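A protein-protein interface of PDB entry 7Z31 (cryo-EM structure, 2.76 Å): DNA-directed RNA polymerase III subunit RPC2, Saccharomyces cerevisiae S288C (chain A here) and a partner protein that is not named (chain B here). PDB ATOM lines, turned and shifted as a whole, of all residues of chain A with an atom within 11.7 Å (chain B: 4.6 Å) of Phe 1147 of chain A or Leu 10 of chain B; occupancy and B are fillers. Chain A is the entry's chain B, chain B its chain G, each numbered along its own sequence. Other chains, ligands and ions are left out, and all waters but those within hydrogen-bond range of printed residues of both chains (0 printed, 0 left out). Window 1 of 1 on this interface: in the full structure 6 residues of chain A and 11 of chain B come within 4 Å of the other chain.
OE1 of Gln 1148 of chain A lies close to OD1 of Asn 69 of chain B, 3.3 Å away.
The backbone NH (N) of Gln 58 of chain B sits at hydrogen-bond distance from the backbone carbonyl oxygen (O) of Tyr 67 of chain B, 2.8 Å away.
Among the printed residues, merely in contact across the chains: Phe 1147 of chain A with Tyr 67 of chain B (3.4 Å), Phe 1147 of chain A with Leu 10 of chain B (3.6 Å), Phe 1147 of chain A with Gln 58 of chain B (3.6 Å), Phe 1147 of chain A with Lys 60 of chain B (3.7 Å), Gln 1148 of chain A with Gln 58 of chain B (3.7 Å) and Phe 1147 of chain A with Leu 59 of chain B (3.96 Å).
Printed residues of chain B within 4 Å of Phe 1147 of chain A: Leu 10 (3.6 Å), Gln 58 (3.6 Å), Leu 59 (3.96 Å), Lys 60 (3.7 Å) and Tyr 67 (3.4 Å). Of the printed residues of chain B, Gln 1148 of chain A touches Gln 58 (3.7 Å) and Asn 69 (3.3 Å). No residue of chain A comes within 4 Å of Asp 9 of chain B. No residue of chain A comes within 4 Å of Val 11 of chain B. Arg 12 of chain B touches none of the printed residues of chain A. Gln 58 of chain B touches just these residues of chain A: Phe 1147 and Gln 1148. Printed residues of chain A within 4 Å of Leu 59 of chain B: Phe 1147 (3.96 Å). Of chain A, only Phe 1147 (3.7 Å) comes within 4 Å of Lys 60 of chain B. Tyr 67 of chain B touches just one residue of chain A: Phe 1147. Of chain A, only Gln 1148 comes within 4 Å of Asn 69 of chain B. The nearest printed residue of chain B that does not touch Phe 1147 of chain A is Asn 69 of chain B (5.0 Å). The nearest residue of chain A that does not touch Leu 10 of chain B is Gln 1148 of chain A (5.6 Å).
Of the 10 printed residues of chain B, 6 touch a printed residue of chain A. Hydrophobic or aromatic side chains of chain A within 4 Å of the printed part of chain B: Phe 1147. Among the printed residues, no Asp or Glu carboxylate lies within 4 Å of a Lys or Arg side-chain nitrogen of the other chain.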
ATOM      1  N   ILE A1117     -39.989  24.319  27.919  1.00  0.00           N
ATOM      2  CA  ILE A1117     -38.602  24.758  27.964  1.00  0.00           C
ATOM      3  C   ILE A1117     -38.591  26.250  28.250  1.00  0.00           C
ATOM      4  O   ILE A1117     -39.538  26.968  27.907  1.00  0.00           O
ATOM      5  CB  ILE A1117     -37.885  24.433  26.641  1.00  0.00           C
ATOM      6  CG1 ILE A1117     -38.051  22.953  26.310  1.00  0.00           C
ATOM      7  CG2 ILE A1117     -36.407  24.796  26.704  1.00  0.00           C
ATOM      8  CD1 ILE A1117     -37.536  22.032  27.389  1.00  0.00           C
ATOM      9  N   LYS A1118     -37.538  26.717  28.904  1.00  0.00           N
ATOM     10  CA  LYS A1118     -37.373  28.128  29.219  1.00  0.00           C
ATOM     11  C   LYS A1118     -36.222  28.669  28.386  1.00  0.00           C
ATOM     12  O   LYS A1118     -35.111  28.130  28.435  1.00  0.00           O
ATOM     13  CB  LYS A1118     -37.111  28.322  30.711  1.00  0.00           C
ATOM     14  CG  LYS A1118     -37.442  29.707  31.217  1.00  0.00           C
ATOM     15  CD  LYS A1118     -37.706  29.687  32.710  1.00  0.00           C
ATOM     16  CE  LYS A1118     -38.060  31.072  33.220  1.00  0.00           C
ATOM     17  NZ  LYS A1118     -39.067  31.741  32.355  1.00  0.00           N
ATOM     18  N   MET A1119     -36.486  29.725  27.623  1.00  0.00           N
ATOM     19  CA  MET A1119     -35.462  30.289  26.758  1.00  0.00           C
ATOM     20  C   MET A1119     -35.704  31.776  26.560  1.00  0.00           C
ATOM     21  O   MET A1119     -36.781  32.297  26.850  1.00  0.00           O
ATOM     22  CB  MET A1119     -35.416  29.584  25.406  1.00  0.00           C
ATOM     23  CG  MET A1119     -36.772  29.331  24.798  1.00  0.00           C
ATOM     24  SD  MET A1119     -36.551  28.449  23.255  1.00  0.00           S
ATOM     25  CE  MET A1119     -35.275  27.302  23.754  1.00  0.00           C
ATOM     26  N   LEU A1143     -37.263  22.783  18.876  1.00  0.00           N
ATOM     27  CA  LEU A1143     -36.082  23.021  19.687  1.00  0.00           C
ATOM     28  C   LEU A1143     -35.126  21.844  19.579  1.00  0.00           C
ATOM     29  O   LEU A1143     -35.408  20.841  18.922  1.00  0.00           O
ATOM     30  CB  LEU A1143     -36.472  23.263  21.148  1.00  0.00           C
ATOM     31  CG  LEU A1143     -37.522  24.341  21.399  1.00  0.00           C
ATOM     32  CD1 LEU A1143     -37.746  24.503  22.878  1.00  0.00           C
ATOM     33  CD2 LEU A1143     -37.108  25.654  20.788  1.00  0.00           C
ATOM     34  N   GLU A1144     -33.975  21.989  20.228  1.00  0.00           N
ATOM     35  CA  GLU A1144     -33.001  20.913  20.335  1.00  0.00           C
ATOM     36  C   GLU A1144     -31.959  21.314  21.362  1.00  0.00           C
ATOM     37  O   GLU A1144     -31.705  22.498  21.574  1.00  0.00           O
ATOM     38  CB  GLU A1144     -32.335  20.611  18.996  1.00  0.00           C
ATOM     39  CG  GLU A1144     -31.560  21.764  18.419  1.00  0.00           C
ATOM     40  CD  GLU A1144     -30.742  21.339  17.228  1.00  0.00           C
ATOM     41  OE1 GLU A1144     -30.735  20.127  16.921  1.00  0.00           O
ATOM     42  OE2 GLU A1144     -30.107  22.206  16.594  1.00  0.00           O
ATOM     43  N   ASP A1145     -31.350  20.311  21.988  1.00  0.00           N
ATOM     44  CA  ASP A1145     -30.344  20.594  22.999  1.00  0.00           C
ATOM     45  C   ASP A1145     -29.143  21.286  22.367  1.00  0.00           C
ATOM     46  O   ASP A1145     -28.689  20.913  21.286  1.00  0.00           O
ATOM     47  CB  ASP A1145     -29.913  19.314  23.717  1.00  0.00           C
ATOM     48  CG  ASP A1145     -29.670  18.154  22.769  1.00  0.00           C
ATOM     49  OD1 ASP A1145     -28.994  18.345  21.739  1.00  0.00           O
ATOM     50  OD2 ASP A1145     -30.147  17.037  23.054  1.00  0.00           O
ATOM     51  N   ILE A1146     -28.657  22.331  23.035  1.00  0.00           N
ATOM     52  CA  ILE A1146     -27.467  23.028  22.559  1.00  0.00           C
ATOM     53  C   ILE A1146     -26.264  22.098  22.585  1.00  0.00           C
ATOM     54  O   ILE A1146     -25.462  22.062  21.645  1.00  0.00           O
ATOM     55  CB  ILE A1146     -27.229  24.293  23.399  1.00  0.00           C
ATOM     56  CG1 ILE A1146     -28.432  25.226  23.294  1.00  0.00           C
ATOM     57  CG2 ILE A1146     -25.969  24.992  22.955  1.00  0.00           C
ATOM     58  CD1 ILE A1146     -28.412  26.360  24.278  1.00  0.00           C
ATOM     59  N   PHE A1147     -26.131  21.328  23.651  1.00  0.00           N
ATOM     60  CA  PHE A1147     -25.034  20.396  23.854  1.00  0.00           C
ATOM     61  C   PHE A1147     -25.434  19.023  23.311  1.00  0.00           C
ATOM     62  O   PHE A1147     -26.332  18.916  22.475  1.00  0.00           O
ATOM     63  CB  PHE A1147     -24.650  20.385  25.332  1.00  0.00           C
ATOM     64  CG  PHE A1147     -24.422  21.751  25.887  1.00  0.00           C
ATOM     65  CD1 PHE A1147     -23.416  22.550  25.384  1.00  0.00           C
ATOM     66  CD2 PHE A1147     -25.220  22.248  26.892  1.00  0.00           C
ATOM     67  CE1 PHE A1147     -23.206  23.806  25.879  1.00  0.00           C
ATOM     68  CE2 PHE A1147     -25.008  23.510  27.389  1.00  0.00           C
ATOM     69  CZ  PHE A1147     -24.000  24.287  26.881  1.00  0.00           C
ATOM     70  N   GLN A1148     -24.718  17.978  23.725  1.00  0.00           N
ATOM     71  CA  GLN A1148     -24.900  16.572  23.345  1.00  0.00           C
ATOM     72  C   GLN A1148     -24.271  16.328  21.983  1.00  0.00           C
ATOM     73  O   GLN A1148     -24.350  15.207  21.459  1.00  0.00           O
ATOM     74  CB  GLN A1148     -26.366  16.120  23.341  1.00  0.00           C
ATOM     75  CG  GLN A1148     -26.574  14.606  23.386  1.00  0.00           C
ATOM     76  CD  GLN A1148     -25.825  13.944  24.523  1.00  0.00           C
ATOM     77  OE1 GLN A1148     -24.672  13.544  24.373  1.00  0.00           O
ATOM     78  NE2 GLN A1148     -26.479  13.821  25.670  1.00  0.00           N
ATOM     79  N   GLN A1149     -23.650  17.348  21.399  1.00  0.00           N
ATOM     80  CA  GLN A1149     -22.776  17.178  20.252  1.00  0.00           C
ATOM     81  C   GLN A1149     -23.513  16.622  19.038  1.00  0.00           C
ATOM     82  O   GLN A1149     -23.745  17.339  18.063  1.00  0.00           O
ATOM     83  CB  GLN A1149     -21.607  16.269  20.640  1.00  0.00           C
ATOM     84  CG  GLN A1149     -20.501  16.182  19.620  1.00  0.00           C
ATOM     85  CD  GLN A1149     -19.295  15.465  20.171  1.00  0.00           C
ATOM     86  OE1 GLN A1149     -19.384  14.321  20.613  1.00  0.00           O
ATOM     87  NE2 GLN A1149     -18.160  16.145  20.176  1.00  0.00           N
ATOM     88  N   ASP B   9     -26.246  12.394  32.465  1.00  0.00           N
ATOM     89  CA  ASP B   9     -26.693  13.729  32.811  1.00  0.00           C
ATOM     90  C   ASP B   9     -25.721  14.760  32.264  1.00  0.00           C
ATOM     91  O   ASP B   9     -24.587  14.449  31.894  1.00  0.00           O
ATOM     92  CB  ASP B   9     -26.847  13.896  34.323  1.00  0.00           C
ATOM     93  CG  ASP B   9     -27.879  14.940  34.685  1.00  0.00           C
ATOM     94  OD1 ASP B   9     -28.638  15.367  33.789  1.00  0.00           O
ATOM     95  OD2 ASP B   9     -27.934  15.340  35.865  1.00  0.00           O
ATOM     96  N   LEU B  10     -26.197  15.997  32.216  1.00  0.00           N
ATOM     97  CA  LEU B  10     -25.417  17.151  31.801  1.00  0.00           C
ATOM     98  C   LEU B  10     -25.242  18.054  33.012  1.00  0.00           C
ATOM     99  O   LEU B  10     -26.229  18.526  33.581  1.00  0.00           O
ATOM    100  CB  LEU B  10     -26.122  17.888  30.667  1.00  0.00           C
ATOM    101  CG  LEU B  10     -25.463  19.130  30.089  1.00  0.00           C
ATOM    102  CD1 LEU B  10     -24.260  18.749  29.263  1.00  0.00           C
ATOM    103  CD2 LEU B  10     -26.470  19.876  29.256  1.00  0.00           C
ATOM    104  N   VAL B  11     -23.994  18.307  33.392  1.00  0.00           N
ATOM    105  CA  VAL B  11     -23.667  18.992  34.636  1.00  0.00           C
ATOM    106  C   VAL B  11     -23.019  20.331  34.312  1.00  0.00           C
ATOM    107  O   VAL B  11     -22.027  20.386  33.578  1.00  0.00           O
ATOM    108  CB  VAL B  11     -22.740  18.134  35.514  1.00  0.00           C
ATOM    109  CG1 VAL B  11     -22.115  18.965  36.589  1.00  0.00           C
ATOM    110  CG2 VAL B  11     -23.507  16.988  36.117  1.00  0.00           C
ATOM    111  N   ARG B  12     -23.565  21.405  34.880  1.00  0.00           N
ATOM    112  CA  ARG B  12     -23.054  22.752  34.663  1.00  0.00           C
ATOM    113  C   ARG B  12     -22.067  23.091  35.774  1.00  0.00           C
ATOM    114  O   ARG B  12     -22.459  23.244  36.934  1.00  0.00           O
ATOM    115  CB  ARG B  12     -24.204  23.754  34.622  1.00  0.00           C
ATOM    116  CG  ARG B  12     -23.754  25.181  34.427  1.00  0.00           C
ATOM    117  CD  ARG B  12     -24.883  26.159  34.634  1.00  0.00           C
ATOM    118  NE  ARG B  12     -24.392  27.442  35.115  1.00  0.00           N
ATOM    119  CZ  ARG B  12     -24.299  27.768  36.396  1.00  0.00           C
ATOM    120  NH1 ARG B  12     -24.671  26.929  37.350  1.00  0.00           N
ATOM    121  NH2 ARG B  12     -23.822  28.962  36.729  1.00  0.00           N
ATOM    122  N   GLN B  58     -18.385  21.502  27.561  1.00  0.00           N
ATOM    123  CA  GLN B  58     -18.694  22.444  26.501  1.00  0.00           C
ATOM    124  C   GLN B  58     -19.163  23.762  27.089  1.00  0.00           C
ATOM    125  O   GLN B  58     -19.612  23.835  28.234  1.00  0.00           O
ATOM    126  CB  GLN B  58     -19.765  21.889  25.566  1.00  0.00           C
ATOM    127  CG  GLN B  58     -19.481  20.496  25.081  1.00  0.00           C
ATOM    128  CD  GLN B  58     -20.664  19.897  24.376  1.00  0.00           C
ATOM    129  OE1 GLN B  58     -21.346  19.032  24.915  1.00  0.00           O
ATOM    130  NE2 GLN B  58     -20.923  20.360  23.160  1.00  0.00           N
ATOM    131  N   LEU B  59     -19.055  24.810  26.283  1.00  0.00           N
ATOM    132  CA  LEU B  59     -19.485  26.143  26.669  1.00  0.00           C
ATOM    133  C   LEU B  59     -20.479  26.673  25.650  1.00  0.00           C
ATOM    134  O   LEU B  59     -20.223  26.628  24.444  1.00  0.00           O
ATOM    135  CB  LEU B  59     -18.293  27.092  26.786  1.00  0.00           C
ATOM    136  CG  LEU B  59     -17.316  26.799  27.921  1.00  0.00           C
ATOM    137  CD1 LEU B  59     -16.080  26.092  27.422  1.00  0.00           C
ATOM    138  CD2 LEU B  59     -16.944  28.075  28.622  1.00  0.00           C
ATOM    139  N   LYS B  60     -21.606  27.151  26.133  1.00  0.00           N
ATOM    140  CA  LYS B  60     -22.495  27.928  25.291  1.00  0.00           C
ATOM    141  C   LYS B  60     -21.956  29.352  25.177  1.00  0.00           C
ATOM    142  O   LYS B  60     -21.216  29.811  26.050  1.00  0.00           O
ATOM    143  CB  LYS B  60     -23.906  27.933  25.867  1.00  0.00           C
ATOM    144  CG  LYS B  60     -23.971  28.410  27.290  1.00  0.00           C
ATOM    145  CD  LYS B  60     -25.235  27.966  27.980  1.00  0.00           C
ATOM    146  CE  LYS B  60     -26.464  28.351  27.203  1.00  0.00           C
ATOM    147  NZ  LYS B  60     -27.681  27.972  27.966  1.00  0.00           N
ATOM    148  N   TYR B  67     -20.242  22.797  30.758  1.00  0.00           N
ATOM    149  CA  TYR B  67     -21.299  21.794  30.789  1.00  0.00           C
ATOM    150  C   TYR B  67     -20.717  20.455  30.362  1.00  0.00           C
ATOM    151  O   TYR B  67     -20.253  20.315  29.229  1.00  0.00           O
ATOM    152  CB  TYR B  67     -22.446  22.174  29.857  1.00  0.00           C
ATOM    153  CG  TYR B  67     -23.242  23.384  30.267  1.00  0.00           C
ATOM    154  CD1 TYR B  67     -22.783  24.665  30.007  1.00  0.00           C
ATOM    155  CD2 TYR B  67     -24.468  23.244  30.884  1.00  0.00           C
ATOM    156  CE1 TYR B  67     -23.516  25.764  30.366  1.00  0.00           C
ATOM    157  CE2 TYR B  67     -25.210  24.333  31.241  1.00  0.00           C
ATOM    158  CZ  TYR B  67     -24.732  25.591  30.982  1.00  0.00           C
ATOM    159  OH  TYR B  67     -25.478  26.685  31.350  1.00  0.00           O
ATOM    160  N   ILE B  68     -20.765  19.469  31.248  1.00  0.00           N
ATOM    161  CA  ILE B  68     -20.151  18.167  31.013  1.00  0.00           C
ATOM    162  C   ILE B  68     -21.242  17.113  30.888  1.00  0.00           C
ATOM    163  O   ILE B  68     -22.113  17.012  31.756  1.00  0.00           O
ATOM    164  CB  ILE B  68     -19.170  17.806  32.140  1.00  0.00           C
ATOM    165  CG1 ILE B  68     -18.070  18.858  32.238  1.00  0.00           C
ATOM    166  CG2 ILE B  68     -18.579  16.446  31.906  1.00  0.00           C
ATOM    167  CD1 ILE B  68     -17.032  18.546  33.249  1.00  0.00           C
ATOM    168  N   ASN B  69     -21.194  16.334  29.809  1.00  0.00           N
ATOM    169  CA  ASN B  69     -22.016  15.133  29.697  1.00  0.00           C
ATOM    170  C   ASN B  69     -21.376  14.030  30.525  1.00  0.00           C
ATOM    171  O   ASN B  69     -20.230  13.648  30.273  1.00  0.00           O
ATOM    172  CB  ASN B  69     -22.153  14.691  28.244  1.00  0.00           C
ATOM    173  CG  ASN B  69     -23.302  15.363  27.537  1.00  0.00           C
ATOM    174  OD1 ASN B  69     -23.189  15.753  26.377  1.00  0.00           O
ATOM    175  ND2 ASN B  69     -24.419  15.510  28.234  1.00  0.00           N
